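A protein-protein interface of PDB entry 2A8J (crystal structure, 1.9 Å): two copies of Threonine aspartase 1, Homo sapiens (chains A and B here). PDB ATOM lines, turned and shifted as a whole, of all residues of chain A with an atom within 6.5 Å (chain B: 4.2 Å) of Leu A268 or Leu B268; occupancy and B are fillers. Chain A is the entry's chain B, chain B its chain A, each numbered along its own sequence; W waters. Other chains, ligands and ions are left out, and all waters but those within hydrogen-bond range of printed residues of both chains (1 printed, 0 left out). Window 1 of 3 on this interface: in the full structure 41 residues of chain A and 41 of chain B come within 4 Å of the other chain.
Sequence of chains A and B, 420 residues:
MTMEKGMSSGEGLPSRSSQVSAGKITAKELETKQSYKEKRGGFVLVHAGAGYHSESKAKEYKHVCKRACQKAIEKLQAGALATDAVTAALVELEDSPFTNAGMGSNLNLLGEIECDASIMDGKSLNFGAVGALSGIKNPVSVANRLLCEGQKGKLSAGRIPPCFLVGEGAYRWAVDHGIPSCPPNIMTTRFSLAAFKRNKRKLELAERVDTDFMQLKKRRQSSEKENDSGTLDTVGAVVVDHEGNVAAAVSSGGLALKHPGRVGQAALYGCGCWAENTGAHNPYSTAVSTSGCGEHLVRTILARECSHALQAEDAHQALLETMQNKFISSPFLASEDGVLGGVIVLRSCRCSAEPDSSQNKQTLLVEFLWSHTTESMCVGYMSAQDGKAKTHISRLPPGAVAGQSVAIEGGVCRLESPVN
The backbone carbonyl oxygen (O) of Phe B164 is in hydrogen-bond range of the backbone NH (N) of Val A263, at 3.1 Å.
O of Tyr B269 lies within hydrogen-bond range of SG of Cys B271, 3.7 Å away. The side-chain sulfur (SG) of Cys A271 sits at hydrogen-bond distance from the backbone carbonyl oxygen (O) of Tyr A269 (3.8 Å). SG of Cys A271 is in hydrogen-bond range of O of Val A298 (3.8 Å).
Among the printed residues, pairs that only touch across the chains: Phe A164 with Leu B268, Leu A268 with Phe B164, Leu A268 with Leu B268, Tyr A269 with Val B298 and Val A298 with Tyr B269.
Of the printed residues of chain B, Val A263 touches Phe B164 (3.1 Å). Of chain B, only Phe B164 (3.7 Å) and Leu B268 (3.9 Å) come within 4 Å of Leu A268. Printed residues of chain B within 4 Å of Val A298: Tyr B269. Of the printed residues of chain A, Phe B164 touches Val A263 and Leu A268. Leu B268 touches just these residues of chain A: Phe A164 (3.8 Å) and Leu A268 (3.9 Å). Of the printed residues of chain A, Val B298 touches Tyr A269 (3.3 Å). The nearest printed residue of chain B that does not touch Leu A268 is Tyr B269 (5.0 Å).
Of the 20 printed residues of chain A, 5 touch a printed residue of chain B. Printed residues of chain A that touch a printed residue of chain B: Phe A164, Val A263, Leu A268, Tyr A269 and Val A298. Along chain B the printed residues that touch a printed residue of chain A span positions 164 to 298. Among the printed residues, no Asp or Glu carboxylate lies within 4 Å of a Lys or Arg side-chain nitrogen of the other chain.
Phe A164 touches Leu B268, and with the chains exchanged Leu A268 touches Phe B164. Leu A268 touches its own counterpart, Leu B268. Tyr A269 touches Val B298, and with the chains exchanged Val A298 touches Tyr B269. 11 positions are printed for both chains. Of the 6 pairs that touch across the chains among the printed residues, 5 have their exchanged pair printed and touching as well.
Water W1 bridges the backbone carbonyl oxygen (O) of Val A263 (2.9 Å) and the backbone NH (N) of Phe B164 (3.1 Å).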
ATOM      1  N   ASP A 116       8.831  -2.276  18.267  1.00  0.00           N
ATOM      2  CA  ASP A 116       9.030  -2.048  19.692  1.00  0.00           C
ATOM      3  C   ASP A 116      10.538  -2.063  19.944  1.00  0.00           C
ATOM      4  O   ASP A 116      11.271  -2.826  19.313  1.00  0.00           O
ATOM      5  CB  ASP A 116       8.401  -3.164  20.534  1.00  0.00           C
ATOM      6  CG  ASP A 116       6.912  -3.333  20.283  1.00  0.00           C
ATOM      7  OD1 ASP A 116       6.266  -2.366  19.824  1.00  0.00           O
ATOM      8  OD2 ASP A 116       6.391  -4.437  20.564  1.00  0.00           O
ATOM      9  N   ALA A 117      11.002  -1.233  20.871  1.00  0.00           N
ATOM     10  CA  ALA A 117      12.424  -1.204  21.185  1.00  0.00           C
ATOM     11  C   ALA A 117      12.663  -0.487  22.498  1.00  0.00           C
ATOM     12  O   ALA A 117      11.921   0.428  22.854  1.00  0.00           O
ATOM     13  CB  ALA A 117      13.203  -0.513  20.054  1.00  0.00           C
ATOM     14  N   SER A 118      13.693  -0.917  23.222  1.00  0.00           N
ATOM     15  CA  SER A 118      14.055  -0.282  24.485  1.00  0.00           C
ATOM     16  C   SER A 118      15.563  -0.366  24.725  1.00  0.00           C
ATOM     17  O   SER A 118      16.264  -1.182  24.121  1.00  0.00           O
ATOM     18  CB  SER A 118      13.293  -0.914  25.658  1.00  0.00           C
ATOM     19  OG  SER A 118      13.533  -2.301  25.750  1.00  0.00           O
ATOM     20  N   PHE A 127      16.183   4.674  31.458  1.00  0.00           N
ATOM     21  CA  PHE A 127      15.610   3.779  30.461  1.00  0.00           C
ATOM     22  C   PHE A 127      14.885   4.561  29.382  1.00  0.00           C
ATOM     23  O   PHE A 127      14.420   5.674  29.624  1.00  0.00           O
ATOM     24  CB  PHE A 127      14.641   2.853  31.207  1.00  0.00           C
ATOM     25  CG  PHE A 127      13.807   1.962  30.331  1.00  0.00           C
ATOM     26  CD1 PHE A 127      14.329   0.775  29.821  1.00  0.00           C
ATOM     27  CD2 PHE A 127      12.464   2.255  30.104  1.00  0.00           C
ATOM     28  CE1 PHE A 127      13.515  -0.117  29.102  1.00  0.00           C
ATOM     29  CE2 PHE A 127      11.641   1.371  29.385  1.00  0.00           C
ATOM     30  CZ  PHE A 127      12.171   0.183  28.888  1.00  0.00           C
ATOM     31  N   ALA A 129      12.186   3.722  25.789  1.00  0.00           N
ATOM     32  CA  ALA A 129      11.485   2.722  24.980  1.00  0.00           C
ATOM     33  C   ALA A 129      10.414   3.301  24.084  1.00  0.00           C
ATOM     34  O   ALA A 129       9.855   4.364  24.364  1.00  0.00           O
ATOM     35  CB  ALA A 129      10.846   1.650  25.891  1.00  0.00           C
ATOM     36  N   VAL A 130      10.131   2.570  23.012  1.00  0.00           N
ATOM     37  CA  VAL A 130       9.094   2.933  22.055  1.00  0.00           C
ATOM     38  C   VAL A 130       8.267   1.693  21.735  1.00  0.00           C
ATOM     39  O   VAL A 130       8.805   0.598  21.617  1.00  0.00           O
ATOM     40  CB  VAL A 130       9.688   3.490  20.735  1.00  0.00           C
ATOM     41  CG1 VAL A 130      10.307   4.865  20.990  1.00  0.00           C
ATOM     42  CG2 VAL A 130      10.720   2.526  20.173  1.00  0.00           C
ATOM     43  N   CYS A 163       9.738   8.300  29.325  1.00  0.00           N
ATOM     44  CA  CYS A 163      10.682   7.240  29.003  1.00  0.00           C
ATOM     45  C   CYS A 163      10.075   6.236  28.031  1.00  0.00           C
ATOM     46  O   CYS A 163      10.791   5.481  27.388  1.00  0.00           O
ATOM     47  CB  CYS A 163      11.159   6.517  30.271  1.00  0.00           C
ATOM     48  SG  CYS A 163       9.930   5.523  31.151  1.00  0.00           S
ATOM     49  N   PHE A 164       8.753   6.259  27.896  1.00  0.00           N
ATOM     50  CA  PHE A 164       8.066   5.315  27.019  1.00  0.00           C
ATOM     51  C   PHE A 164       6.975   5.991  26.204  1.00  0.00           C
ATOM     52  O   PHE A 164       5.990   6.482  26.770  1.00  0.00           O
ATOM     53  CB  PHE A 164       7.477   4.184  27.884  1.00  0.00           C
ATOM     54  CG  PHE A 164       6.722   3.120  27.109  1.00  0.00           C
ATOM     55  CD1 PHE A 164       7.130   2.726  25.840  1.00  0.00           C
ATOM     56  CD2 PHE A 164       5.624   2.476  27.688  1.00  0.00           C
ATOM     57  CE1 PHE A 164       6.457   1.701  25.147  1.00  0.00           C
ATOM     58  CE2 PHE A 164       4.946   1.449  27.008  1.00  0.00           C
ATOM     59  CZ  PHE A 164       5.367   1.062  25.735  1.00  0.00           C
ATOM     60  N   VAL A 263       1.712  -4.507  21.588  1.00  0.00           N
ATOM     61  CA  VAL A 263       3.052  -4.211  22.068  1.00  0.00           C
ATOM     62  C   VAL A 263       3.573  -5.401  22.837  1.00  0.00           C
ATOM     63  O   VAL A 263       2.878  -5.956  23.699  1.00  0.00           O
ATOM     64  CB  VAL A 263       3.039  -2.951  22.978  1.00  0.00           C
ATOM     65  CG1 VAL A 263       4.424  -2.690  23.560  1.00  0.00           C
ATOM     66  CG2 VAL A 263       2.569  -1.753  22.168  1.00  0.00           C
ATOM     67  N   GLY A 264       4.801  -5.787  22.512  1.00  0.00           N
ATOM     68  CA  GLY A 264       5.426  -6.923  23.159  1.00  0.00           C
ATOM     69  C   GLY A 264       6.561  -6.581  24.115  1.00  0.00           C
ATOM     70  O   GLY A 264       6.733  -5.440  24.548  1.00  0.00           O
ATOM     71  N   GLN A 265       7.349  -7.600  24.421  1.00  0.00           N
ATOM     72  CA  GLN A 265       8.469  -7.501  25.343  1.00  0.00           C
ATOM     73  C   GLN A 265       9.576  -6.492  25.016  1.00  0.00           C
ATOM     74  O   GLN A 265      10.164  -5.925  25.934  1.00  0.00           O
ATOM     75  CB  GLN A 265       9.078  -8.892  25.506  1.00  0.00           C
ATOM     76  CG  GLN A 265       9.555  -9.481  24.170  1.00  0.00           C
ATOM     77  CD  GLN A 265      11.020  -9.249  23.940  1.00  0.00           C
ATOM     78  OE1 GLN A 265      11.539  -9.509  22.864  1.00  0.00           O
ATOM     79  NE2 GLN A 265      11.706  -8.768  24.965  1.00  0.00           N
ATOM     80  N   ALA A 266       9.869  -6.256  23.738  1.00  0.00           N
ATOM     81  CA  ALA A 266      10.948  -5.325  23.390  1.00  0.00           C
ATOM     82  C   ALA A 266      10.714  -3.879  23.836  1.00  0.00           C
ATOM     83  O   ALA A 266      11.643  -3.070  23.852  1.00  0.00           O
ATOM     84  CB  ALA A 266      11.215  -5.355  21.885  1.00  0.00           C
ATOM     85  N   ALA A 267       9.481  -3.556  24.202  1.00  0.00           N
ATOM     86  CA  ALA A 267       9.143  -2.195  24.616  1.00  0.00           C
ATOM     87  C   ALA A 267       8.940  -2.057  26.112  1.00  0.00           C
ATOM     88  O   ALA A 267       8.838  -0.947  26.629  1.00  0.00           O
ATOM     89  CB  ALA A 267       7.864  -1.740  23.896  1.00  0.00           C
ATOM     90  N   LEU A 268       8.885  -3.178  26.810  1.00  0.00           N
ATOM     91  CA  LEU A 268       8.594  -3.126  28.230  1.00  0.00           C
ATOM     92  C   LEU A 268       9.748  -3.208  29.209  1.00  0.00           C
ATOM     93  O   LEU A 268      10.584  -4.109  29.148  1.00  0.00           O
ATOM     94  CB  LEU A 268       7.546  -4.191  28.577  1.00  0.00           C
ATOM     95  CG  LEU A 268       6.218  -4.088  27.816  1.00  0.00           C
ATOM     96  CD1 LEU A 268       5.206  -5.043  28.452  1.00  0.00           C
ATOM     97  CD2 LEU A 268       5.685  -2.668  27.876  1.00  0.00           C
ATOM     98  N   TYR A 269       9.754  -2.245  30.125  1.00  0.00           N
ATOM     99  CA  TYR A 269      10.758  -2.140  31.174  1.00  0.00           C
ATOM    100  C   TYR A 269      10.837  -3.443  31.958  1.00  0.00           C
ATOM    101  O   TYR A 269       9.811  -4.000  32.358  1.00  0.00           O
ATOM    102  CB  TYR A 269      10.388  -0.986  32.115  1.00  0.00           C
ATOM    103  CG  TYR A 269      11.412  -0.688  33.201  1.00  0.00           C
ATOM    104  CD1 TYR A 269      12.599  -0.014  32.912  1.00  0.00           C
ATOM    105  CD2 TYR A 269      11.170  -1.053  34.526  1.00  0.00           C
ATOM    106  CE1 TYR A 269      13.523   0.296  33.930  1.00  0.00           C
ATOM    107  CE2 TYR A 269      12.075  -0.750  35.540  1.00  0.00           C
ATOM    108  CZ  TYR A 269      13.250  -0.071  35.239  1.00  0.00           C
ATOM    109  OH  TYR A 269      14.118   0.233  36.269  1.00  0.00           O
ATOM    110  N   GLY A 270      12.058  -3.923  32.169  1.00  0.00           N
ATOM    111  CA  GLY A 270      12.265  -5.152  32.915  1.00  0.00           C
ATOM    112  C   GLY A 270      12.070  -6.439  32.131  1.00  0.00           C
ATOM    113  O   GLY A 270      12.531  -7.487  32.550  1.00  0.00           O
ATOM    114  N   CYS A 271      11.409  -6.359  30.984  1.00  0.00           N
ATOM    115  CA  CYS A 271      11.134  -7.543  30.178  1.00  0.00           C
ATOM    116  C   CYS A 271      12.071  -7.787  28.998  1.00  0.00           C
ATOM    117  O   CYS A 271      12.627  -8.878  28.860  1.00  0.00           O
ATOM    118  CB  CYS A 271       9.684  -7.485  29.685  1.00  0.00           C
ATOM    119  SG  CYS A 271       8.484  -7.290  31.026  1.00  0.00           S
ATOM    120  N   GLY A 272      12.241  -6.774  28.156  1.00  0.00           N
ATOM    121  CA  GLY A 272      13.084  -6.896  26.980  1.00  0.00           C
ATOM    122  C   GLY A 272      14.582  -6.810  27.241  1.00  0.00           C
ATOM    123  O   GLY A 272      15.346  -7.572  26.655  1.00  0.00           O
ATOM    124  N   CYS A 273      15.010  -5.865  28.080  1.00  0.00           N
ATOM    125  CA  CYS A 273      16.425  -5.733  28.411  1.00  0.00           C
ATOM    126  C   CYS A 273      16.591  -5.171  29.815  1.00  0.00           C
ATOM    127  O   CYS A 273      15.642  -4.652  30.401  1.00  0.00           O
ATOM    128  CB  CYS A 273      17.152  -4.830  27.395  1.00  0.00           C
ATOM    129  SG  CYS A 273      16.723  -3.074  27.441  1.00  0.00           S
ATOM    130  N   VAL A 298       7.295 -11.300  28.798  1.00  0.00           N
ATOM    131  CA  VAL A 298       6.644 -10.283  29.618  1.00  0.00           C
ATOM    132  C   VAL A 298       6.110 -10.815  30.950  1.00  0.00           C
ATOM    133  O   VAL A 298       6.432 -10.281  32.006  1.00  0.00           O
ATOM    134  CB  VAL A 298       5.483  -9.613  28.848  1.00  0.00           C
ATOM    135  CG1 VAL A 298       4.642  -8.750  29.794  1.00  0.00           C
ATOM    136  CG2 VAL A 298       6.055  -8.763  27.717  1.00  0.00           C
ATOM    137  N   PHE B 164      -1.467  -6.670  25.799  1.00  0.00           N
ATOM    138  CA  PHE B 164      -1.234  -5.232  25.848  1.00  0.00           C
ATOM    139  C   PHE B 164      -1.384  -4.570  24.483  1.00  0.00           C
ATOM    140  O   PHE B 164      -0.602  -4.824  23.561  1.00  0.00           O
ATOM    141  CB  PHE B 164       0.168  -4.983  26.426  1.00  0.00           C
ATOM    142  CG  PHE B 164       0.531  -3.518  26.604  1.00  0.00           C
ATOM    143  CD1 PHE B 164      -0.441  -2.559  26.869  1.00  0.00           C
ATOM    144  CD2 PHE B 164       1.864  -3.118  26.554  1.00  0.00           C
ATOM    145  CE1 PHE B 164      -0.089  -1.206  27.084  1.00  0.00           C
ATOM    146  CE2 PHE B 164       2.229  -1.775  26.770  1.00  0.00           C
ATOM    147  CZ  PHE B 164       1.243  -0.822  27.034  1.00  0.00           C
ATOM    148  N   GLY B 264       2.152   5.489  30.997  1.00  0.00           N
ATOM    149  CA  GLY B 264       2.599   5.388  32.376  1.00  0.00           C
ATOM    150  C   GLY B 264       2.450   4.016  33.010  1.00  0.00           C
ATOM    151  O   GLY B 264       2.193   3.021  32.329  1.00  0.00           O
ATOM    152  N   GLN B 265       2.593   3.974  34.330  1.00  0.00           N
ATOM    153  CA  GLN B 265       2.532   2.726  35.077  1.00  0.00           C
ATOM    154  C   GLN B 265       1.207   1.969  35.049  1.00  0.00           C
ATOM    155  O   GLN B 265       1.205   0.746  35.169  1.00  0.00           O
ATOM    156  CB  GLN B 265       2.982   2.969  36.532  1.00  0.00           C
ATOM    157  CG  GLN B 265       1.940   2.720  37.610  1.00  0.00           C
ATOM    158  CD  GLN B 265       0.943   3.860  37.737  1.00  0.00           C
ATOM    159  OE1 GLN B 265       1.065   4.887  37.068  1.00  0.00           O
ATOM    160  NE2 GLN B 265      -0.045   3.682  38.605  1.00  0.00           N
ATOM    161  N   ALA B 266       0.091   2.671  34.882  1.00  0.00           N
ATOM    162  CA  ALA B 266      -1.219   2.006  34.865  1.00  0.00           C
ATOM    163  C   ALA B 266      -1.397   0.991  33.729  1.00  0.00           C
ATOM    164  O   ALA B 266      -2.290   0.138  33.768  1.00  0.00           O
ATOM    165  CB  ALA B 266      -2.329   3.047  34.806  1.00  0.00           C
ATOM    166  N   ALA B 267      -0.548   1.090  32.718  1.00  0.00           N
ATOM    167  CA  ALA B 267      -0.608   0.183  31.587  1.00  0.00           C
ATOM    168  C   ALA B 267       0.499  -0.875  31.620  1.00  0.00           C
ATOM    169  O   ALA B 267       0.453  -1.853  30.864  1.00  0.00           O
ATOM    170  CB  ALA B 267      -0.510   0.978  30.294  1.00  0.00           C
ATOM    171  N   LEU B 268       1.473  -0.708  32.510  1.00  0.00           N
ATOM    172  CA  LEU B 268       2.614  -1.628  32.543  1.00  0.00           C
ATOM    173  C   LEU B 268       2.605  -2.793  33.535  1.00  0.00           C
ATOM    174  O   LEU B 268       2.507  -2.600  34.750  1.00  0.00           O
ATOM    175  CB  LEU B 268       3.903  -0.824  32.729  1.00  0.00           C
ATOM    176  CG  LEU B 268       4.169   0.324  31.746  1.00  0.00           C
ATOM    177  CD1 LEU B 268       5.592   0.809  31.928  1.00  0.00           C
ATOM    178  CD2 LEU B 268       3.972  -0.136  30.317  1.00  0.00           C
ATOM    179  N   TYR B 269       2.754  -4.002  32.990  1.00  0.00           N
ATOM    180  CA  TYR B 269       2.777  -5.241  33.769  1.00  0.00           C
ATOM    181  C   TYR B 269       3.764  -5.131  34.928  1.00  0.00           C
ATOM    182  O   TYR B 269       4.906  -4.718  34.745  1.00  0.00           O
ATOM    183  CB  TYR B 269       3.166  -6.424  32.856  1.00  0.00           C
ATOM    184  CG  TYR B 269       3.132  -7.810  33.492  1.00  0.00           C
ATOM    185  CD1 TYR B 269       1.917  -8.435  33.804  1.00  0.00           C
ATOM    186  CD2 TYR B 269       4.314  -8.509  33.754  1.00  0.00           C
ATOM    187  CE1 TYR B 269       1.885  -9.729  34.359  1.00  0.00           C
ATOM    188  CE2 TYR B 269       4.294  -9.800  34.306  1.00  0.00           C
ATOM    189  CZ  TYR B 269       3.080 -10.403  34.605  1.00  0.00           C
ATOM    190  OH  TYR B 269       3.071 -11.674  35.150  1.00  0.00           O
ATOM    191  N   GLY B 270       3.310  -5.493  36.125  1.00  0.00           N
ATOM    192  CA  GLY B 270       4.171  -5.441  37.300  1.00  0.00           C
ATOM    193  C   GLY B 270       4.271  -4.088  37.989  1.00  0.00           C
ATOM    194  O   GLY B 270       4.630  -4.004  39.166  1.00  0.00           O
ATOM    195  N   CYS B 271       3.924  -3.027  37.268  1.00  0.00           N
ATOM    196  CA  CYS B 271       4.023  -1.680  37.813  1.00  0.00           C
ATOM    197  C   CYS B 271       2.717  -1.067  38.338  1.00  0.00           C
ATOM    198  O   CYS B 271       2.675  -0.550  39.457  1.00  0.00           O
ATOM    199  CB  CYS B 271       4.649  -0.760  36.755  1.00  0.00           C
ATOM    200  SG  CYS B 271       6.145  -1.450  35.971  1.00  0.00           S
ATOM    201  N   GLY B 272       1.659  -1.124  37.537  1.00  0.00           N
ATOM    202  CA  GLY B 272       0.392  -0.545  37.946  1.00  0.00           C
ATOM    203  C   GLY B 272      -0.409  -1.379  38.925  1.00  0.00           C
ATOM    204  O   GLY B 272      -1.036  -0.845  39.834  1.00  0.00           O
ATOM    205  N   VAL B 298       7.126   2.879  37.692  1.00  0.00           N
ATOM    206  CA  VAL B 298       7.632   1.981  36.654  1.00  0.00           C
ATOM    207  C   VAL B 298       9.069   1.534  36.943  1.00  0.00           C
ATOM    208  O   VAL B 298       9.357   0.336  36.974  1.00  0.00           O
ATOM    209  CB  VAL B 298       7.585   2.668  35.258  1.00  0.00           C
ATOM    210  CG1 VAL B 298       8.378   1.849  34.232  1.00  0.00           C
ATOM    211  CG2 VAL B 298       6.138   2.805  34.807  1.00  0.00           C
HETATM  212  O   HOH W   1       0.695  -7.877  23.942  1.00  0.00           O
